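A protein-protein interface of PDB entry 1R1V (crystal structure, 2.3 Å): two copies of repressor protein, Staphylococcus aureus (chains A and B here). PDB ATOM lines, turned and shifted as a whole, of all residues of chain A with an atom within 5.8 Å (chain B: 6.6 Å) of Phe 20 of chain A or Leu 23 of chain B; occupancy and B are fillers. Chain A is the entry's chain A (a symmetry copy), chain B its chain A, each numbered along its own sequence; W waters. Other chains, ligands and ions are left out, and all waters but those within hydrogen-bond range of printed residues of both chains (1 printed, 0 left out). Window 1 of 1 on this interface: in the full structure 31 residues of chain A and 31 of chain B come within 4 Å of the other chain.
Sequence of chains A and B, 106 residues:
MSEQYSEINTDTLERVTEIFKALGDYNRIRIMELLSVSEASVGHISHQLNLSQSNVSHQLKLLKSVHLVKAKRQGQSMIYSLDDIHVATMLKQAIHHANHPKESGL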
ATOM      1  N   ARG A  15      -7.222 -16.893 -31.584  1.00  0.00           N
ATOM      2  CA  ARG A  15      -8.338 -16.415 -30.777  1.00  0.00           C
ATOM      3  C   ARG A  15      -9.356 -17.526 -30.521  1.00  0.00           C
ATOM      4  O   ARG A  15      -9.846 -17.650 -29.407  1.00  0.00           O
ATOM      5  CB  ARG A  15      -9.021 -15.205 -31.432  1.00  0.00           C
ATOM      6  CG  ARG A  15      -8.226 -13.896 -31.311  1.00  0.00           C
ATOM      7  CD  ARG A  15      -9.084 -12.675 -31.645  1.00  0.00           C
ATOM      8  NE  ARG A  15      -9.456 -12.597 -33.059  1.00  0.00           N
ATOM      9  CZ  ARG A  15      -8.755 -11.947 -33.987  1.00  0.00           C
ATOM     10  NH1 ARG A  15      -7.638 -11.306 -33.655  1.00  0.00           N
ATOM     11  NH2 ARG A  15      -9.170 -11.931 -35.249  1.00  0.00           N
ATOM     12  N   VAL A  16      -9.672 -18.335 -31.535  1.00  0.00           N
ATOM     13  CA  VAL A  16     -10.622 -19.435 -31.328  1.00  0.00           C
ATOM     14  C   VAL A  16     -10.014 -20.487 -30.395  1.00  0.00           C
ATOM     15  O   VAL A  16     -10.729 -21.173 -29.678  1.00  0.00           O
ATOM     16  CB  VAL A  16     -11.046 -20.112 -32.662  1.00  0.00           C
ATOM     17  CG1 VAL A  16     -11.877 -19.151 -33.492  1.00  0.00           C
ATOM     18  CG2 VAL A  16      -9.835 -20.539 -33.441  1.00  0.00           C
ATOM     19  N   THR A  17      -8.689 -20.612 -30.416  1.00  0.00           N
ATOM     20  CA  THR A  17      -8.009 -21.550 -29.535  1.00  0.00           C
ATOM     21  C   THR A  17      -8.292 -21.076 -28.109  1.00  0.00           C
ATOM     22  O   THR A  17      -8.621 -21.866 -27.222  1.00  0.00           O
ATOM     23  CB  THR A  17      -6.485 -21.542 -29.777  1.00  0.00           C
ATOM     24  OG1 THR A  17      -6.219 -21.899 -31.137  1.00  0.00           O
ATOM     25  CG2 THR A  17      -5.792 -22.544 -28.867  1.00  0.00           C
ATOM     26  N   GLU A  18      -8.181 -19.765 -27.914  1.00  0.00           N
ATOM     27  CA  GLU A  18      -8.430 -19.134 -26.626  1.00  0.00           C
ATOM     28  C   GLU A  18      -9.831 -19.497 -26.142  1.00  0.00           C
ATOM     29  O   GLU A  18     -10.015 -19.946 -25.010  1.00  0.00           O
ATOM     30  CB  GLU A  18      -8.336 -17.615 -26.768  1.00  0.00           C
ATOM     31  CG  GLU A  18      -7.267 -16.956 -25.926  1.00  0.00           C
ATOM     32  CD  GLU A  18      -5.877 -17.380 -26.325  1.00  0.00           C
ATOM     33  OE1 GLU A  18      -5.553 -18.579 -26.161  1.00  0.00           O
ATOM     34  OE2 GLU A  18      -5.110 -16.512 -26.805  1.00  0.00           O
ATOM     35  N   ILE A  19     -10.814 -19.276 -27.010  1.00  0.00           N
ATOM     36  CA  ILE A  19     -12.206 -19.572 -26.707  1.00  0.00           C
ATOM     37  C   ILE A  19     -12.398 -21.023 -26.247  1.00  0.00           C
ATOM     38  O   ILE A  19     -12.971 -21.271 -25.190  1.00  0.00           O
ATOM     39  CB  ILE A  19     -13.115 -19.300 -27.947  1.00  0.00           C
ATOM     40  CG1 ILE A  19     -13.220 -17.790 -28.187  1.00  0.00           C
ATOM     41  CG2 ILE A  19     -14.517 -19.895 -27.733  1.00  0.00           C
ATOM     42  CD1 ILE A  19     -13.914 -17.410 -29.493  1.00  0.00           C
ATOM     43  N   PHE A  20     -11.908 -21.974 -27.036  1.00  0.00           N
ATOM     44  CA  PHE A  20     -12.061 -23.379 -26.686  1.00  0.00           C
ATOM     45  C   PHE A  20     -11.294 -23.764 -25.429  1.00  0.00           C
ATOM     46  O   PHE A  20     -11.770 -24.581 -24.646  1.00  0.00           O
ATOM     47  CB  PHE A  20     -11.655 -24.279 -27.863  1.00  0.00           C
ATOM     48  CG  PHE A  20     -12.578 -24.170 -29.057  1.00  0.00           C
ATOM     49  CD1 PHE A  20     -13.958 -24.292 -28.902  1.00  0.00           C
ATOM     50  CD2 PHE A  20     -12.069 -23.960 -30.337  1.00  0.00           C
ATOM     51  CE1 PHE A  20     -14.819 -24.205 -30.010  1.00  0.00           C
ATOM     52  CE2 PHE A  20     -12.920 -23.874 -31.448  1.00  0.00           C
ATOM     53  CZ  PHE A  20     -14.295 -23.996 -31.283  1.00  0.00           C
ATOM     54  N   LYS A  21     -10.119 -23.175 -25.220  1.00  0.00           N
ATOM     55  CA  LYS A  21      -9.358 -23.502 -24.018  1.00  0.00           C
ATOM     56  C   LYS A  21     -10.118 -23.060 -22.780  1.00  0.00           C
ATOM     57  O   LYS A  21      -9.954 -23.636 -21.715  1.00  0.00           O
ATOM     58  CB  LYS A  21      -7.969 -22.852 -24.037  1.00  0.00           C
ATOM     59  CG  LYS A  21      -6.921 -23.678 -24.756  1.00  0.00           C
ATOM     60  CD  LYS A  21      -5.546 -23.027 -24.693  1.00  0.00           C
ATOM     61  CE  LYS A  21      -4.478 -23.923 -25.315  1.00  0.00           C
ATOM     62  NZ  LYS A  21      -3.130 -23.274 -25.342  1.00  0.00           N
ATOM     63  N   ALA A  22     -10.963 -22.044 -22.931  1.00  0.00           N
ATOM     64  CA  ALA A  22     -11.763 -21.530 -21.819  1.00  0.00           C
ATOM     65  C   ALA A  22     -12.998 -22.404 -21.543  1.00  0.00           C
ATOM     66  O   ALA A  22     -13.518 -22.432 -20.431  1.00  0.00           O
ATOM     67  CB  ALA A  22     -12.189 -20.085 -22.109  1.00  0.00           C
ATOM     68  N   LEU A  23     -13.465 -23.116 -22.558  1.00  0.00           N
ATOM     69  CA  LEU A  23     -14.626 -23.989 -22.401  1.00  0.00           C
ATOM     70  C   LEU A  23     -14.190 -25.370 -21.922  1.00  0.00           C
ATOM     71  O   LEU A  23     -15.006 -26.154 -21.443  1.00  0.00           O
ATOM     72  CB  LEU A  23     -15.366 -24.141 -23.734  1.00  0.00           C
ATOM     73  CG  LEU A  23     -16.007 -22.883 -24.317  1.00  0.00           C
ATOM     74  CD1 LEU A  23     -16.515 -23.175 -25.711  1.00  0.00           C
ATOM     75  CD2 LEU A  23     -17.138 -22.436 -23.423  1.00  0.00           C
ATOM     76  N   GLY A  24     -12.900 -25.661 -22.064  1.00  0.00           N
ATOM     77  CA  GLY A  24     -12.379 -26.953 -21.655  1.00  0.00           C
ATOM     78  C   GLY A  24     -12.210 -27.094 -20.154  1.00  0.00           C
ATOM     79  O   GLY A  24     -11.127 -27.421 -19.669  1.00  0.00           O
ATOM     80  N   MET A  90     -23.140 -22.428 -30.574  1.00  0.00           N
ATOM     81  CA  MET A  90     -21.917 -23.195 -30.411  1.00  0.00           C
ATOM     82  C   MET A  90     -22.027 -24.184 -29.251  1.00  0.00           C
ATOM     83  O   MET A  90     -21.721 -25.369 -29.396  1.00  0.00           O
ATOM     84  CB  MET A  90     -20.755 -22.241 -30.161  1.00  0.00           C
ATOM     85  CG  MET A  90     -19.462 -22.918 -29.757  1.00  0.00           C
ATOM     86  SD  MET A  90     -18.232 -21.678 -29.362  1.00  0.00           S
ATOM     87  CE  MET A  90     -18.613 -21.410 -27.613  1.00  0.00           C
ATOM     88  N   GLU B  18     -14.546 -32.753 -22.524  1.00  0.00           N
ATOM     89  CA  GLU B  18     -13.594 -33.522 -23.313  1.00  0.00           C
ATOM     90  C   GLU B  18     -13.471 -32.909 -24.705  1.00  0.00           C
ATOM     91  O   GLU B  18     -12.369 -32.639 -25.185  1.00  0.00           O
ATOM     92  CB  GLU B  18     -14.081 -34.964 -23.450  1.00  0.00           C
ATOM     93  CG  GLU B  18     -13.156 -36.013 -22.875  1.00  0.00           C
ATOM     94  CD  GLU B  18     -13.004 -35.889 -21.380  1.00  0.00           C
ATOM     95  OE1 GLU B  18     -12.453 -34.861 -20.924  1.00  0.00           O
ATOM     96  OE2 GLU B  18     -13.439 -36.822 -20.665  1.00  0.00           O
ATOM     97  N   ILE B  19     -14.618 -32.714 -25.350  1.00  0.00           N
ATOM     98  CA  ILE B  19     -14.676 -32.135 -26.683  1.00  0.00           C
ATOM     99  C   ILE B  19     -13.942 -30.790 -26.758  1.00  0.00           C
ATOM    100  O   ILE B  19     -13.075 -30.600 -27.606  1.00  0.00           O
ATOM    101  CB  ILE B  19     -16.156 -31.941 -27.140  1.00  0.00           C
ATOM    102  CG1 ILE B  19     -16.790 -33.307 -27.426  1.00  0.00           C
ATOM    103  CG2 ILE B  19     -16.224 -31.059 -28.399  1.00  0.00           C
ATOM    104  CD1 ILE B  19     -18.295 -33.256 -27.682  1.00  0.00           C
ATOM    105  N   PHE B  20     -14.283 -29.867 -25.863  1.00  0.00           N
ATOM    106  CA  PHE B  20     -13.650 -28.556 -25.872  1.00  0.00           C
ATOM    107  C   PHE B  20     -12.168 -28.611 -25.531  1.00  0.00           C
ATOM    108  O   PHE B  20     -11.381 -27.854 -26.094  1.00  0.00           O
ATOM    109  CB  PHE B  20     -14.386 -27.592 -24.930  1.00  0.00           C
ATOM    110  CG  PHE B  20     -15.787 -27.247 -25.387  1.00  0.00           C
ATOM    111  CD1 PHE B  20     -16.023 -26.810 -26.690  1.00  0.00           C
ATOM    112  CD2 PHE B  20     -16.868 -27.346 -24.513  1.00  0.00           C
ATOM    113  CE1 PHE B  20     -17.320 -26.475 -27.115  1.00  0.00           C
ATOM    114  CE2 PHE B  20     -18.165 -27.012 -24.928  1.00  0.00           C
ATOM    115  CZ  PHE B  20     -18.389 -26.578 -26.230  1.00  0.00           C
ATOM    116  N   LYS B  21     -11.776 -29.505 -24.627  1.00  0.00           N
ATOM    117  CA  LYS B  21     -10.361 -29.604 -24.283  1.00  0.00           C
ATOM    118  C   LYS B  21      -9.558 -30.054 -25.491  1.00  0.00           C
ATOM    119  O   LYS B  21      -8.383 -29.739 -25.604  1.00  0.00           O
ATOM    120  CB  LYS B  21     -10.131 -30.570 -23.114  1.00  0.00           C
ATOM    121  CG  LYS B  21     -10.274 -29.920 -21.751  1.00  0.00           C
ATOM    122  CD  LYS B  21      -9.973 -30.899 -20.624  1.00  0.00           C
ATOM    123  CE  LYS B  21     -10.004 -30.206 -19.265  1.00  0.00           C
ATOM    124  NZ  LYS B  21      -9.793 -31.159 -18.131  1.00  0.00           N
ATOM    125  N   ALA B  22     -10.204 -30.779 -26.399  1.00  0.00           N
ATOM    126  CA  ALA B  22      -9.547 -31.265 -27.613  1.00  0.00           C
ATOM    127  C   ALA B  22      -9.438 -30.171 -28.688  1.00  0.00           C
ATOM    128  O   ALA B  22      -8.561 -30.213 -29.546  1.00  0.00           O
ATOM    129  CB  ALA B  22     -10.307 -32.479 -28.164  1.00  0.00           C
ATOM    130  N   LEU B  23     -10.331 -29.194 -28.640  1.00  0.00           N
ATOM    131  CA  LEU B  23     -10.309 -28.098 -29.605  1.00  0.00           C
ATOM    132  C   LEU B  23      -9.389 -26.981 -29.121  1.00  0.00           C
ATOM    133  O   LEU B  23      -8.991 -26.116 -29.898  1.00  0.00           O
ATOM    134  CB  LEU B  23     -11.718 -27.527 -29.800  1.00  0.00           C
ATOM    135  CG  LEU B  23     -12.763 -28.455 -30.415  1.00  0.00           C
ATOM    136  CD1 LEU B  23     -14.123 -27.799 -30.348  1.00  0.00           C
ATOM    137  CD2 LEU B  23     -12.387 -28.755 -31.846  1.00  0.00           C
ATOM    138  N   GLY B  24      -9.064 -27.006 -27.833  1.00  0.00           N
ATOM    139  CA  GLY B  24      -8.207 -25.983 -27.262  1.00  0.00           C
ATOM    140  C   GLY B  24      -6.739 -26.162 -27.599  1.00  0.00           C
ATOM    141  O   GLY B  24      -5.888 -26.212 -26.711  1.00  0.00           O
ATOM    142  N   ASP B  25      -6.440 -26.251 -28.887  1.00  0.00           N
ATOM    143  CA  ASP B  25      -5.071 -26.424 -29.354  1.00  0.00           C
ATOM    144  C   ASP B  25      -4.957 -25.779 -30.726  1.00  0.00           C
ATOM    145  O   ASP B  25      -5.751 -26.063 -31.621  1.00  0.00           O
ATOM    146  CB  ASP B  25      -4.725 -27.916 -29.435  1.00  0.00           C
ATOM    147  CG  ASP B  25      -3.323 -28.166 -29.954  1.00  0.00           C
ATOM    148  OD1 ASP B  25      -3.138 -28.273 -31.186  1.00  0.00           O
ATOM    149  OD2 ASP B  25      -2.400 -28.252 -29.126  1.00  0.00           O
ATOM    150  N   TYR B  26      -3.962 -24.918 -30.888  1.00  0.00           N
ATOM    151  CA  TYR B  26      -3.772 -24.214 -32.145  1.00  0.00           C
ATOM    152  C   TYR B  26      -3.728 -25.118 -33.371  1.00  0.00           C
ATOM    153  O   TYR B  26      -4.453 -24.889 -34.337  1.00  0.00           O
ATOM    154  CB  TYR B  26      -2.504 -23.371 -32.080  1.00  0.00           C
ATOM    155  CG  TYR B  26      -2.261 -22.561 -33.328  1.00  0.00           C
ATOM    156  CD1 TYR B  26      -3.172 -21.592 -33.739  1.00  0.00           C
ATOM    157  CD2 TYR B  26      -1.112 -22.758 -34.094  1.00  0.00           C
ATOM    158  CE1 TYR B  26      -2.944 -20.834 -34.886  1.00  0.00           C
ATOM    159  CE2 TYR B  26      -0.873 -22.005 -35.241  1.00  0.00           C
ATOM    160  CZ  TYR B  26      -1.788 -21.050 -35.630  1.00  0.00           C
ATOM    161  OH  TYR B  26      -1.552 -20.313 -36.766  1.00  0.00           O
ATOM    162  N   ARG B  28      -4.730 -28.291 -33.648  1.00  0.00           N
ATOM    163  CA  ARG B  28      -5.912 -29.119 -33.835  1.00  0.00           C
ATOM    164  C   ARG B  28      -6.994 -28.242 -34.458  1.00  0.00           C
ATOM    165  O   ARG B  28      -7.824 -28.714 -35.229  1.00  0.00           O
ATOM    166  CB  ARG B  28      -6.386 -29.725 -32.504  1.00  0.00           C
ATOM    167  CG  ARG B  28      -5.406 -30.749 -31.927  1.00  0.00           C
ATOM    168  CD  ARG B  28      -6.087 -31.759 -31.008  1.00  0.00           C
ATOM    169  NE  ARG B  28      -6.310 -31.259 -29.655  1.00  0.00           N
ATOM    170  CZ  ARG B  28      -5.366 -31.153 -28.725  1.00  0.00           C
ATOM    171  NH1 ARG B  28      -4.121 -31.512 -28.987  1.00  0.00           N
ATOM    172  NH2 ARG B  28      -5.669 -30.678 -27.527  1.00  0.00           N
ATOM    173  N   ILE B  29      -6.961 -26.954 -34.133  1.00  0.00           N
ATOM    174  CA  ILE B  29      -7.916 -26.007 -34.685  1.00  0.00           C
ATOM    175  C   ILE B  29      -7.610 -25.835 -36.173  1.00  0.00           C
ATOM    176  O   ILE B  29      -8.522 -25.775 -36.992  1.00  0.00           O
ATOM    177  CB  ILE B  29      -7.828 -24.640 -33.967  1.00  0.00           C
ATOM    178  CG1 ILE B  29      -8.370 -24.772 -32.540  1.00  0.00           C
ATOM    179  CG2 ILE B  29      -8.633 -23.589 -34.729  1.00  0.00           C
ATOM    180  CD1 ILE B  29      -9.847 -25.124 -32.476  1.00  0.00           C
ATOM    181  N   MET B  32      -8.975 -28.883 -37.869  1.00  0.00           N
ATOM    182  CA  MET B  32     -10.434 -28.853 -37.944  1.00  0.00           C
ATOM    183  C   MET B  32     -10.907 -27.859 -39.005  1.00  0.00           C
ATOM    184  O   MET B  32     -11.773 -28.168 -39.834  1.00  0.00           O
ATOM    185  CB  MET B  32     -11.006 -28.473 -36.582  1.00  0.00           C
ATOM    186  CG  MET B  32     -10.717 -29.499 -35.501  1.00  0.00           C
ATOM    187  SD  MET B  32     -11.649 -31.008 -35.798  1.00  0.00           S
ATOM    188  CE  MET B  32     -13.230 -30.487 -35.147  1.00  0.00           C
ATOM    189  N   LEU B  63      -8.728 -36.370 -31.787  1.00  0.00           N
ATOM    190  CA  LEU B  63      -9.953 -35.769 -32.294  1.00  0.00           C
ATOM    191  C   LEU B  63     -11.021 -36.821 -32.570  1.00  0.00           C
ATOM    192  O   LEU B  63     -12.208 -36.592 -32.314  1.00  0.00           O
ATOM    193  CB  LEU B  63      -9.661 -34.952 -33.558  1.00  0.00           C
ATOM    194  CG  LEU B  63      -8.870 -33.669 -33.277  1.00  0.00           C
ATOM    195  CD1 LEU B  63      -8.465 -32.973 -34.576  1.00  0.00           C
ATOM    196  CD2 LEU B  63      -9.717 -32.753 -32.420  1.00  0.00           C
ATOM    197  N   LEU B  68     -14.992 -35.880 -32.886  1.00  0.00           N
ATOM    198  CA  LEU B  68     -14.942 -34.585 -33.553  1.00  0.00           C
ATOM    199  C   LEU B  68     -14.666 -34.804 -35.038  1.00  0.00           C
ATOM    200  O   LEU B  68     -15.092 -34.009 -35.884  1.00  0.00           O
ATOM    201  CB  LEU B  68     -13.854 -33.692 -32.932  1.00  0.00           C
ATOM    202  CG  LEU B  68     -14.200 -33.119 -31.549  1.00  0.00           C
ATOM    203  CD1 LEU B  68     -13.061 -32.287 -31.019  1.00  0.00           C
ATOM    204  CD2 LEU B  68     -15.461 -32.282 -31.655  1.00  0.00           C
ATOM    205  N   VAL B  87     -20.692 -30.675 -35.420  1.00  0.00           N
ATOM    206  CA  VAL B  87     -19.295 -30.303 -35.275  1.00  0.00           C
ATOM    207  C   VAL B  87     -18.976 -29.128 -36.189  1.00  0.00           C
ATOM    208  O   VAL B  87     -18.309 -28.183 -35.782  1.00  0.00           O
ATOM    209  CB  VAL B  87     -18.366 -31.490 -35.622  1.00  0.00           C
ATOM    210  CG1 VAL B  87     -16.905 -31.059 -35.532  1.00  0.00           C
ATOM    211  CG2 VAL B  87     -18.640 -32.659 -34.676  1.00  0.00           C
ATOM    212  N   MET B  90     -20.754 -25.957 -34.903  1.00  0.00           N
ATOM    213  CA  MET B  90     -20.047 -25.567 -33.695  1.00  0.00           C
ATOM    214  C   MET B  90     -18.761 -24.808 -34.019  1.00  0.00           C
ATOM    215  O   MET B  90     -18.504 -23.732 -33.474  1.00  0.00           O
ATOM    216  CB  MET B  90     -19.714 -26.813 -32.883  1.00  0.00           C
ATOM    217  CG  MET B  90     -18.788 -26.569 -31.710  1.00  0.00           C
ATOM    218  SD  MET B  90     -18.373 -28.131 -30.937  1.00  0.00           S
ATOM    219  CE  MET B  90     -16.943 -28.603 -31.941  1.00  0.00           C
ATOM    220  N   LEU B  91     -17.962 -25.376 -34.913  1.00  0.00           N
ATOM    221  CA  LEU B  91     -16.698 -24.774 -35.312  1.00  0.00           C
ATOM    222  C   LEU B  91     -16.861 -23.457 -36.078  1.00  0.00           C
ATOM    223  O   LEU B  91     -16.214 -22.464 -35.752  1.00  0.00           O
ATOM    224  CB  LEU B  91     -15.909 -25.760 -36.171  1.00  0.00           C
ATOM    225  CG  LEU B  91     -14.527 -25.293 -36.606  1.00  0.00           C
ATOM    226  CD1 LEU B  91     -13.615 -25.221 -35.384  1.00  0.00           C
ATOM    227  CD2 LEU B  91     -13.964 -26.251 -37.634  1.00  0.00           C
ATOM    228  N   ALA B  94     -17.992 -20.561 -33.965  1.00  0.00           N
ATOM    229  CA  ALA B  94     -16.906 -20.062 -33.119  1.00  0.00           C
ATOM    230  C   ALA B  94     -15.923 -19.215 -33.913  1.00  0.00           C
ATOM    231  O   ALA B  94     -15.521 -18.158 -33.443  1.00  0.00           O
ATOM    232  CB  ALA B  94     -16.166 -21.219 -32.438  1.00  0.00           C
ATOM    233  N   ILE B  95     -15.547 -19.680 -35.106  1.00  0.00           N
ATOM    234  CA  ILE B  95     -14.612 -18.948 -35.966  1.00  0.00           C
ATOM    235  C   ILE B  95     -15.154 -17.554 -36.225  1.00  0.00           C
ATOM    236  O   ILE B  95     -14.444 -16.561 -36.084  1.00  0.00           O
ATOM    237  CB  ILE B  95     -14.422 -19.642 -37.336  1.00  0.00           C
ATOM    238  CG1 ILE B  95     -13.782 -21.018 -37.144  1.00  0.00           C
ATOM    239  CG2 ILE B  95     -13.536 -18.790 -38.246  1.00  0.00           C
ATOM    240  CD1 ILE B  95     -12.452 -20.969 -36.437  1.00  0.00           C
HETATM  241  O   HOH W   1     -19.426 -19.621 -31.178  1.00  0.00           O
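The guanidinium group (NH2) of Arg 28 of chain B is in hydrogen-bond range of the backbone carbonyl oxygen (O) of Lys 21 of chain B, at 3.5 Å. The side-chain carboxylate (OD2) of Asp 25 of chain B lies within salt-bridge range of the guanidinium group (NH1) of Arg 28 of chain B (3.7 Å).
Phe 20 of chain A touches its own counterpart, Phe 20 of chain B. Phe 20 of chain A touches Leu 23 of chain B, and with the chains exchanged Leu 23 of chain A touches Phe 20 of chain B. Phe 20 of chain A touches Gly 24 of chain B, and with the chains exchanged Gly 24 of chain A touches Phe 20 of chain B. Lys 21 of chain A touches Gly 24 of chain B, and with the chains exchanged Gly 24 of chain A touches Lys 21 of chain B. Positions printed for both chains: 18, 19, 20, 21, 22, 23, 24 and 90. Of the 18 pairs that touch across the chains among the printed residues, 8 have their exchanged pair printed and touching as well.
Val 16 of chain A touches Ile 29 of chain B (CG2 to CG2, 3.5 Å). Thr 17 of chain A touches Gly 24 of chain B (CG2 to C, 3.9 Å). Thr 17 of chain A touches Tyr 26 of chain B (OG1 to CA, 3.5 Å). OG1 of Thr 17 of chain A touches CG1 of Ile 29 of chain B, at 3.9 Å. N of Gly 24 of chain B touches CB of Phe 20 of chain A, 3.8 Å away. Gly 24 of chain B touches Lys 21 of chain A (O to CE, 3.0 Å). CB of Leu 23 of chain A touches CG of Phe 20 of chain B, at 3.5 Å. Gly 24 of chain A touches Phe 20 of chain B. CG of Met 90 of chain A touches O of Met 90 of chain B, at 3.9 Å. Ala 94 of chain B touches Met 90 of chain A (CB to SD, 3.7 Å).
Of the 11 printed residues of chain A, 7 touch a printed residue of chain B. Among the printed residues, no Asp or Glu carboxylate lies within 4 Å of a Lys or Arg side-chain nitrogen of the other chain.
Printed residues of chain B within 4 Å of Val 16 of chain A: Ile 29, Ala 94 and Ile 95. Of the printed residues of chain B, Gly 24 of chain A touches Phe 20 and Lys 21. Glu 18 of chain B touches none of the printed residues of chain A. Printed residues of chain A within 4 Å of Asp 25 of chain B: Thr 17. Leu 91 of chain B touches none of the printed residues of chain A. The nearest printed residue of chain A that does not touch Asp 25 of chain B is Lys 21 of chain A (4.7 Å).
Water W1 bridges SD of Met 90 of chain A (3.0 Å) and N of Ala 94 of chain B (3.3 Å).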
